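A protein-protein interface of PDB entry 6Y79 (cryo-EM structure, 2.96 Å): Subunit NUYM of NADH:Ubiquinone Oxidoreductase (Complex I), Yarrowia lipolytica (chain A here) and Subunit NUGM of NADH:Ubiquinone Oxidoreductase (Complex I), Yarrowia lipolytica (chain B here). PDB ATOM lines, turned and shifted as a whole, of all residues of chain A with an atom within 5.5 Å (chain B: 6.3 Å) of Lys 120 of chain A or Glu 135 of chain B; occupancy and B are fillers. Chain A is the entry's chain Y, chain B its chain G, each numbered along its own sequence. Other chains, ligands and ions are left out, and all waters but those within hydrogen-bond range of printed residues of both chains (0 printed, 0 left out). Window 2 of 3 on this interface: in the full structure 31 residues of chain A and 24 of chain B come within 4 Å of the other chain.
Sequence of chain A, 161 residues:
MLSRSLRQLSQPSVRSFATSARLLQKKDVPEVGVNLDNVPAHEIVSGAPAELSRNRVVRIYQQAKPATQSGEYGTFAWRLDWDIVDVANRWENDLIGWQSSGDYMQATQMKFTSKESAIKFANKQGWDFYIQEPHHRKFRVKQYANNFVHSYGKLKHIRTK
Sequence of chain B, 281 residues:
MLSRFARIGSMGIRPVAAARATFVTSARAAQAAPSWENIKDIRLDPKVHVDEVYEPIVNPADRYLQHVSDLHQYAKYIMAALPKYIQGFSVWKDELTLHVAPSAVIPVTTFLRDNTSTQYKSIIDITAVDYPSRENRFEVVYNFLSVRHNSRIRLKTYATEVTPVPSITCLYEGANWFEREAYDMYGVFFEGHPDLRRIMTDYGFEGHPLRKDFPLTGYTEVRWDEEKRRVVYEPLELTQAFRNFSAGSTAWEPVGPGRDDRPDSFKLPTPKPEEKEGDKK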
ATOM      1  N   LYS A 115     -13.908  -7.932 -12.938  1.00  0.00           N
ATOM      2  CA  LYS A 115     -13.535  -8.579 -11.685  1.00  0.00           C
ATOM      3  C   LYS A 115     -14.599  -8.354 -10.622  1.00  0.00           C
ATOM      4  O   LYS A 115     -14.953  -9.271  -9.866  1.00  0.00           O
ATOM      5  CB  LYS A 115     -12.188  -8.039 -11.222  1.00  0.00           C
ATOM      6  CG  LYS A 115     -11.746  -8.485  -9.864  1.00  0.00           C
ATOM      7  CD  LYS A 115     -10.318  -8.058  -9.600  1.00  0.00           C
ATOM      8  CE  LYS A 115     -10.231  -6.576  -9.304  1.00  0.00           C
ATOM      9  NZ  LYS A 115     -10.772  -6.273  -7.956  1.00  0.00           N
ATOM     10  N   GLU A 116     -15.154  -7.143 -10.582  1.00  0.00           N
ATOM     11  CA  GLU A 116     -16.201  -6.836  -9.619  1.00  0.00           C
ATOM     12  C   GLU A 116     -17.507  -7.527  -9.990  1.00  0.00           C
ATOM     13  O   GLU A 116     -18.317  -7.832  -9.107  1.00  0.00           O
ATOM     14  CB  GLU A 116     -16.380  -5.321  -9.507  1.00  0.00           C
ATOM     15  CG  GLU A 116     -15.215  -4.608  -8.816  1.00  0.00           C
ATOM     16  CD  GLU A 116     -14.065  -4.250  -9.751  1.00  0.00           C
ATOM     17  OE1 GLU A 116     -14.184  -4.496 -10.970  1.00  0.00           O
ATOM     18  OE2 GLU A 116     -13.047  -3.710  -9.264  1.00  0.00           O
ATOM     19  N   SER A 117     -17.711  -7.815 -11.285  1.00  0.00           N
ATOM     20  CA  SER A 117     -18.811  -8.683 -11.708  1.00  0.00           C
ATOM     21  C   SER A 117     -18.698 -10.061 -11.082  1.00  0.00           C
ATOM     22  O   SER A 117     -19.672 -10.580 -10.524  1.00  0.00           O
ATOM     23  CB  SER A 117     -18.847  -8.821 -13.228  1.00  0.00           C
ATOM     24  OG  SER A 117     -19.201  -7.611 -13.880  1.00  0.00           O
ATOM     25  N   ALA A 118     -17.509 -10.659 -11.151  1.00  0.00           N
ATOM     26  CA  ALA A 118     -17.297 -11.996 -10.607  1.00  0.00           C
ATOM     27  C   ALA A 118     -17.438 -12.013  -9.094  1.00  0.00           C
ATOM     28  O   ALA A 118     -18.033 -12.939  -8.538  1.00  0.00           O
ATOM     29  CB  ALA A 118     -15.923 -12.527 -11.021  1.00  0.00           C
ATOM     30  N   ILE A 119     -16.934 -10.975  -8.415  1.00  0.00           N
ATOM     31  CA  ILE A 119     -17.057 -10.902  -6.959  1.00  0.00           C
ATOM     32  C   ILE A 119     -18.513 -10.709  -6.539  1.00  0.00           C
ATOM     33  O   ILE A 119     -18.984 -11.358  -5.594  1.00  0.00           O
ATOM     34  CB  ILE A 119     -16.156  -9.786  -6.403  1.00  0.00           C
ATOM     35  CG1 ILE A 119     -14.691 -10.075  -6.687  1.00  0.00           C
ATOM     36  CG2 ILE A 119     -16.314  -9.647  -4.912  1.00  0.00           C
ATOM     37  CD1 ILE A 119     -13.811  -8.893  -6.409  1.00  0.00           C
ATOM     38  N   LYS A 120     -19.250  -9.830  -7.238  1.00  0.00           N
ATOM     39  CA  LYS A 120     -20.653  -9.575  -6.914  1.00  0.00           C
ATOM     40  C   LYS A 120     -21.503 -10.816  -7.114  1.00  0.00           C
ATOM     41  O   LYS A 120     -22.347 -11.142  -6.271  1.00  0.00           O
ATOM     42  CB  LYS A 120     -21.197  -8.434  -7.770  1.00  0.00           C
ATOM     43  CG  LYS A 120     -20.937  -7.052  -7.217  1.00  0.00           C
ATOM     44  CD  LYS A 120     -21.291  -5.986  -8.231  1.00  0.00           C
ATOM     45  CE  LYS A 120     -20.753  -4.628  -7.812  1.00  0.00           C
ATOM     46  NZ  LYS A 120     -21.154  -3.559  -8.763  1.00  0.00           N
ATOM     47  N   PHE A 121     -21.267 -11.542  -8.209  1.00  0.00           N
ATOM     48  CA  PHE A 121     -21.984 -12.789  -8.437  1.00  0.00           C
ATOM     49  C   PHE A 121     -21.568 -13.864  -7.438  1.00  0.00           C
ATOM     50  O   PHE A 121     -22.389 -14.694  -7.042  1.00  0.00           O
ATOM     51  CB  PHE A 121     -21.750 -13.262  -9.871  1.00  0.00           C
ATOM     52  CG  PHE A 121     -22.525 -14.491 -10.236  1.00  0.00           C
ATOM     53  CD1 PHE A 121     -23.837 -14.396 -10.645  1.00  0.00           C
ATOM     54  CD2 PHE A 121     -21.943 -15.742 -10.164  1.00  0.00           C
ATOM     55  CE1 PHE A 121     -24.547 -15.518 -10.968  1.00  0.00           C
ATOM     56  CE2 PHE A 121     -22.657 -16.857 -10.467  1.00  0.00           C
ATOM     57  CZ  PHE A 121     -23.954 -16.748 -10.875  1.00  0.00           C
ATOM     58  N   ALA A 122     -20.301 -13.870  -7.023  1.00  0.00           N
ATOM     59  CA  ALA A 122     -19.811 -14.956  -6.185  1.00  0.00           C
ATOM     60  C   ALA A 122     -20.302 -14.826  -4.754  1.00  0.00           C
ATOM     61  O   ALA A 122     -20.650 -15.831  -4.122  1.00  0.00           O
ATOM     62  CB  ALA A 122     -18.287 -15.006  -6.224  1.00  0.00           C
ATOM     63  N   ASN A 123     -20.333 -13.609  -4.210  1.00  0.00           N
ATOM     64  CA  ASN A 123     -20.895 -13.470  -2.874  1.00  0.00           C
ATOM     65  C   ASN A 123     -22.404 -13.271  -2.892  1.00  0.00           C
ATOM     66  O   ASN A 123     -23.039 -13.365  -1.839  1.00  0.00           O
ATOM     67  CB  ASN A 123     -20.190 -12.352  -2.078  1.00  0.00           C
ATOM     68  CG  ASN A 123     -20.252 -10.987  -2.741  1.00  0.00           C
ATOM     69  OD1 ASN A 123     -21.021 -10.741  -3.664  1.00  0.00           O
ATOM     70  ND2 ASN A 123     -19.421 -10.081  -2.255  1.00  0.00           N
ATOM     71  N   LYS A 124     -22.988 -13.008  -4.061  1.00  0.00           N
ATOM     72  CA  LYS A 124     -24.437 -13.016  -4.192  1.00  0.00           C
ATOM     73  C   LYS A 124     -24.993 -14.432  -4.134  1.00  0.00           C
ATOM     74  O   LYS A 124     -26.093 -14.651  -3.621  1.00  0.00           O
ATOM     75  CB  LYS A 124     -24.832 -12.338  -5.497  1.00  0.00           C
ATOM     76  CG  LYS A 124     -26.296 -12.083  -5.652  1.00  0.00           C
ATOM     77  CD  LYS A 124     -26.584 -11.398  -6.963  1.00  0.00           C
ATOM     78  CE  LYS A 124     -26.047  -9.987  -6.969  1.00  0.00           C
ATOM     79  NZ  LYS A 124     -26.478  -9.258  -8.191  1.00  0.00           N
ATOM     80  N   GLN A 125     -24.255 -15.402  -4.659  1.00  0.00           N
ATOM     81  CA  GLN A 125     -24.636 -16.803  -4.552  1.00  0.00           C
ATOM     82  C   GLN A 125     -24.156 -17.440  -3.259  1.00  0.00           C
ATOM     83  O   GLN A 125     -24.423 -18.622  -3.037  1.00  0.00           O
ATOM     84  CB  GLN A 125     -24.091 -17.595  -5.741  1.00  0.00           C
ATOM     85  CG  GLN A 125     -24.637 -17.185  -7.092  1.00  0.00           C
ATOM     86  CD  GLN A 125     -26.127 -17.366  -7.200  1.00  0.00           C
ATOM     87  OE1 GLN A 125     -26.865 -16.412  -7.439  1.00  0.00           O
ATOM     88  NE2 GLN A 125     -26.586 -18.594  -7.015  1.00  0.00           N
ATOM     89  N   TYR B 131     -26.969 -13.303 -18.586  1.00  0.00           N
ATOM     90  CA  TYR B 131     -25.607 -12.805 -18.593  1.00  0.00           C
ATOM     91  C   TYR B 131     -25.236 -12.631 -17.136  1.00  0.00           C
ATOM     92  O   TYR B 131     -25.733 -11.698 -16.495  1.00  0.00           O
ATOM     93  CB  TYR B 131     -25.487 -11.477 -19.340  1.00  0.00           C
ATOM     94  CG  TYR B 131     -25.685 -11.527 -20.844  1.00  0.00           C
ATOM     95  CD1 TYR B 131     -25.937 -12.707 -21.498  1.00  0.00           C
ATOM     96  CD2 TYR B 131     -25.566 -10.387 -21.611  1.00  0.00           C
ATOM     97  CE1 TYR B 131     -26.114 -12.748 -22.842  1.00  0.00           C
ATOM     98  CE2 TYR B 131     -25.732 -10.431 -22.975  1.00  0.00           C
ATOM     99  CZ  TYR B 131     -26.007 -11.628 -23.577  1.00  0.00           C
ATOM    100  OH  TYR B 131     -26.182 -11.749 -24.927  1.00  0.00           O
ATOM    101  N   PRO B 132     -24.421 -13.509 -16.547  1.00  0.00           N
ATOM    102  CA  PRO B 132     -24.141 -13.393 -15.109  1.00  0.00           C
ATOM    103  C   PRO B 132     -23.267 -12.205 -14.737  1.00  0.00           C
ATOM    104  O   PRO B 132     -23.161 -11.895 -13.546  1.00  0.00           O
ATOM    105  CB  PRO B 132     -23.449 -14.722 -14.783  1.00  0.00           C
ATOM    106  CG  PRO B 132     -22.890 -15.180 -16.064  1.00  0.00           C
ATOM    107  CD  PRO B 132     -23.833 -14.728 -17.122  1.00  0.00           C
ATOM    108  N   SER B 133     -22.661 -11.522 -15.705  1.00  0.00           N
ATOM    109  CA  SER B 133     -21.827 -10.368 -15.412  1.00  0.00           C
ATOM    110  C   SER B 133     -22.626  -9.085 -15.245  1.00  0.00           C
ATOM    111  O   SER B 133     -22.052  -8.067 -14.848  1.00  0.00           O
ATOM    112  CB  SER B 133     -20.786 -10.187 -16.511  1.00  0.00           C
ATOM    113  OG  SER B 133     -21.380 -10.309 -17.787  1.00  0.00           O
ATOM    114  N   ARG B 134     -23.919  -9.101 -15.535  1.00  0.00           N
ATOM    115  CA  ARG B 134     -24.764  -7.932 -15.354  1.00  0.00           C
ATOM    116  C   ARG B 134     -25.432  -7.953 -13.984  1.00  0.00           C
ATOM    117  O   ARG B 134     -25.552  -9.006 -13.353  1.00  0.00           O
ATOM    118  CB  ARG B 134     -25.820  -7.871 -16.451  1.00  0.00           C
ATOM    119  CG  ARG B 134     -25.248  -7.527 -17.790  1.00  0.00           C
ATOM    120  CD  ARG B 134     -26.322  -7.344 -18.822  1.00  0.00           C
ATOM    121  NE  ARG B 134     -27.108  -8.553 -18.965  1.00  0.00           N
ATOM    122  CZ  ARG B 134     -28.020  -8.750 -19.908  1.00  0.00           C
ATOM    123  NH1 ARG B 134     -28.262  -7.818 -20.819  1.00  0.00           N
ATOM    124  NH2 ARG B 134     -28.675  -9.901 -19.948  1.00  0.00           N
ATOM    125  N   GLU B 135     -25.844  -6.764 -13.519  1.00  0.00           N
ATOM    126  CA  GLU B 135     -26.622  -6.674 -12.284  1.00  0.00           C
ATOM    127  C   GLU B 135     -27.959  -7.381 -12.437  1.00  0.00           C
ATOM    128  O   GLU B 135     -28.321  -8.234 -11.619  1.00  0.00           O
ATOM    129  CB  GLU B 135     -26.871  -5.216 -11.894  1.00  0.00           C
ATOM    130  CG  GLU B 135     -25.656  -4.385 -11.520  1.00  0.00           C
ATOM    131  CD  GLU B 135     -24.985  -4.823 -10.237  1.00  0.00           C
ATOM    132  OE1 GLU B 135     -25.683  -5.336  -9.343  1.00  0.00           O
ATOM    133  OE2 GLU B 135     -23.758  -4.637 -10.119  1.00  0.00           O
ATOM    134  N   ASN B 136     -28.700  -7.033 -13.479  1.00  0.00           N
ATOM    135  CA  ASN B 136     -29.942  -7.709 -13.826  1.00  0.00           C
ATOM    136  C   ASN B 136     -29.570  -8.869 -14.734  1.00  0.00           C
ATOM    137  O   ASN B 136     -29.216  -8.675 -15.897  1.00  0.00           O
ATOM    138  CB  ASN B 136     -30.907  -6.736 -14.483  1.00  0.00           C
ATOM    139  CG  ASN B 136     -31.373  -5.669 -13.528  1.00  0.00           C
ATOM    140  OD1 ASN B 136     -32.270  -5.892 -12.723  1.00  0.00           O
ATOM    141  ND2 ASN B 136     -30.750  -4.505 -13.596  1.00  0.00           N
ATOM    142  N   ARG B 137     -29.662 -10.080 -14.185  1.00  0.00           N
ATOM    143  CA  ARG B 137     -28.969 -11.239 -14.737  1.00  0.00           C
ATOM    144  C   ARG B 137     -29.591 -11.700 -16.042  1.00  0.00           C
ATOM    145  O   ARG B 137     -28.889 -11.941 -17.027  1.00  0.00           O
ATOM    146  CB  ARG B 137     -28.992 -12.362 -13.706  1.00  0.00           C
ATOM    147  CG  ARG B 137     -28.356 -13.636 -14.142  1.00  0.00           C
ATOM    148  CD  ARG B 137     -28.407 -14.639 -13.027  1.00  0.00           C
ATOM    149  NE  ARG B 137     -27.599 -15.807 -13.336  1.00  0.00           N
ATOM    150  CZ  ARG B 137     -27.461 -16.849 -12.532  1.00  0.00           C
ATOM    151  NH1 ARG B 137     -28.082 -16.868 -11.365  1.00  0.00           N
ATOM    152  NH2 ARG B 137     -26.704 -17.869 -12.897  1.00  0.00           N
ATOM    153  N   PHE B 138     -30.906 -11.824 -16.067  1.00  0.00           N
ATOM    154  CA  PHE B 138     -31.622 -12.342 -17.216  1.00  0.00           C
ATOM    155  C   PHE B 138     -32.099 -11.200 -18.086  1.00  0.00           C
ATOM    156  O   PHE B 138     -32.472 -10.144 -17.587  1.00  0.00           O
ATOM    157  CB  PHE B 138     -32.812 -13.177 -16.754  1.00  0.00           C
ATOM    158  CG  PHE B 138     -32.419 -14.353 -15.934  1.00  0.00           C
ATOM    159  CD1 PHE B 138     -31.995 -15.507 -16.541  1.00  0.00           C
ATOM    160  CD2 PHE B 138     -32.440 -14.299 -14.557  1.00  0.00           C
ATOM    161  CE1 PHE B 138     -31.619 -16.591 -15.791  1.00  0.00           C
ATOM    162  CE2 PHE B 138     -32.056 -15.381 -13.811  1.00  0.00           C
ATOM    163  CZ  PHE B 138     -31.630 -16.517 -14.432  1.00  0.00           C
ATOM    164  N   ALA B 159     -34.507  -8.769 -16.144  1.00  0.00           N
ATOM    165  CA  ALA B 159     -35.019  -9.312 -14.895  1.00  0.00           C
ATOM    166  C   ALA B 159     -33.862  -9.825 -14.065  1.00  0.00           C
ATOM    167  O   ALA B 159     -32.970 -10.484 -14.593  1.00  0.00           O
ATOM    168  CB  ALA B 159     -35.989 -10.456 -15.136  1.00  0.00           C
ATOM    169  N   THR B 160     -33.884  -9.533 -12.776  1.00  0.00           N
ATOM    170  CA  THR B 160     -33.037 -10.253 -11.848  1.00  0.00           C
ATOM    171  C   THR B 160     -33.743 -11.551 -11.458  1.00  0.00           C
ATOM    172  O   THR B 160     -34.931 -11.736 -11.718  1.00  0.00           O
ATOM    173  CB  THR B 160     -32.720  -9.368 -10.633  1.00  0.00           C
ATOM    174  OG1 THR B 160     -32.500  -8.029 -11.086  1.00  0.00           O
ATOM    175  CG2 THR B 160     -31.443  -9.800  -9.899  1.00  0.00           C
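The backbone carbonyl oxygen of Ser 133 of chain B is in hydrogen-bond range of the side-chain hydroxyl of Ser 117 of chain A (3.0 Å).
The side-chain amino group (NZ) of Lys 120 of chain A is in salt-bridge range of the side-chain carboxylate (OE2) of Glu 135 of chain B (3.1 Å).
Printed residues of chain B that touch a printed residue of chain A: Pro 132, Ser 133, Glu 135 and Arg 137.
The backbone carbonyl oxygen of Lys 120 of chain A sits close to the side-chain amide oxygen of Asn 123 of chain A (3.0 Å).
The backbone carbonyl oxygen of Arg 137 of chain B sits at hydrogen-bond distance from the backbone NH of Tyr 131 of chain B (2.8 Å).
N of Arg 137 of chain B lies within hydrogen-bond range of O of Ala 159 of chain B (3.4 Å).
Printed residues of chain B within 4 Å of Lys 120 of chain A: Glu 135.
Glu 135 of chain B touches just one residue of chain A: Lys 120 (3.1 Å).
Of the printed residues of chain A, Pro 132 of chain B touches Phe 121.
Printed residues of chain A within 4 Å of Ser 133 of chain B: Ser 117 (3.0 Å).
Of the printed residues of chain B, Ser 117 of chain A touches Ser 133 (3.0 Å).
Lys 115 of chain A touches none of the printed residues of chain B.
Ala 118 of chain A touches none of the printed residues of chain B.
The nearest residue of chain A that does not touch Glu 135 of chain B is Lys 124 of chain A (4.02 Å).
Phe 121 of chain A touches Pro 132 of chain B.
Arg 137 of chain B touches Phe 121 of chain A.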
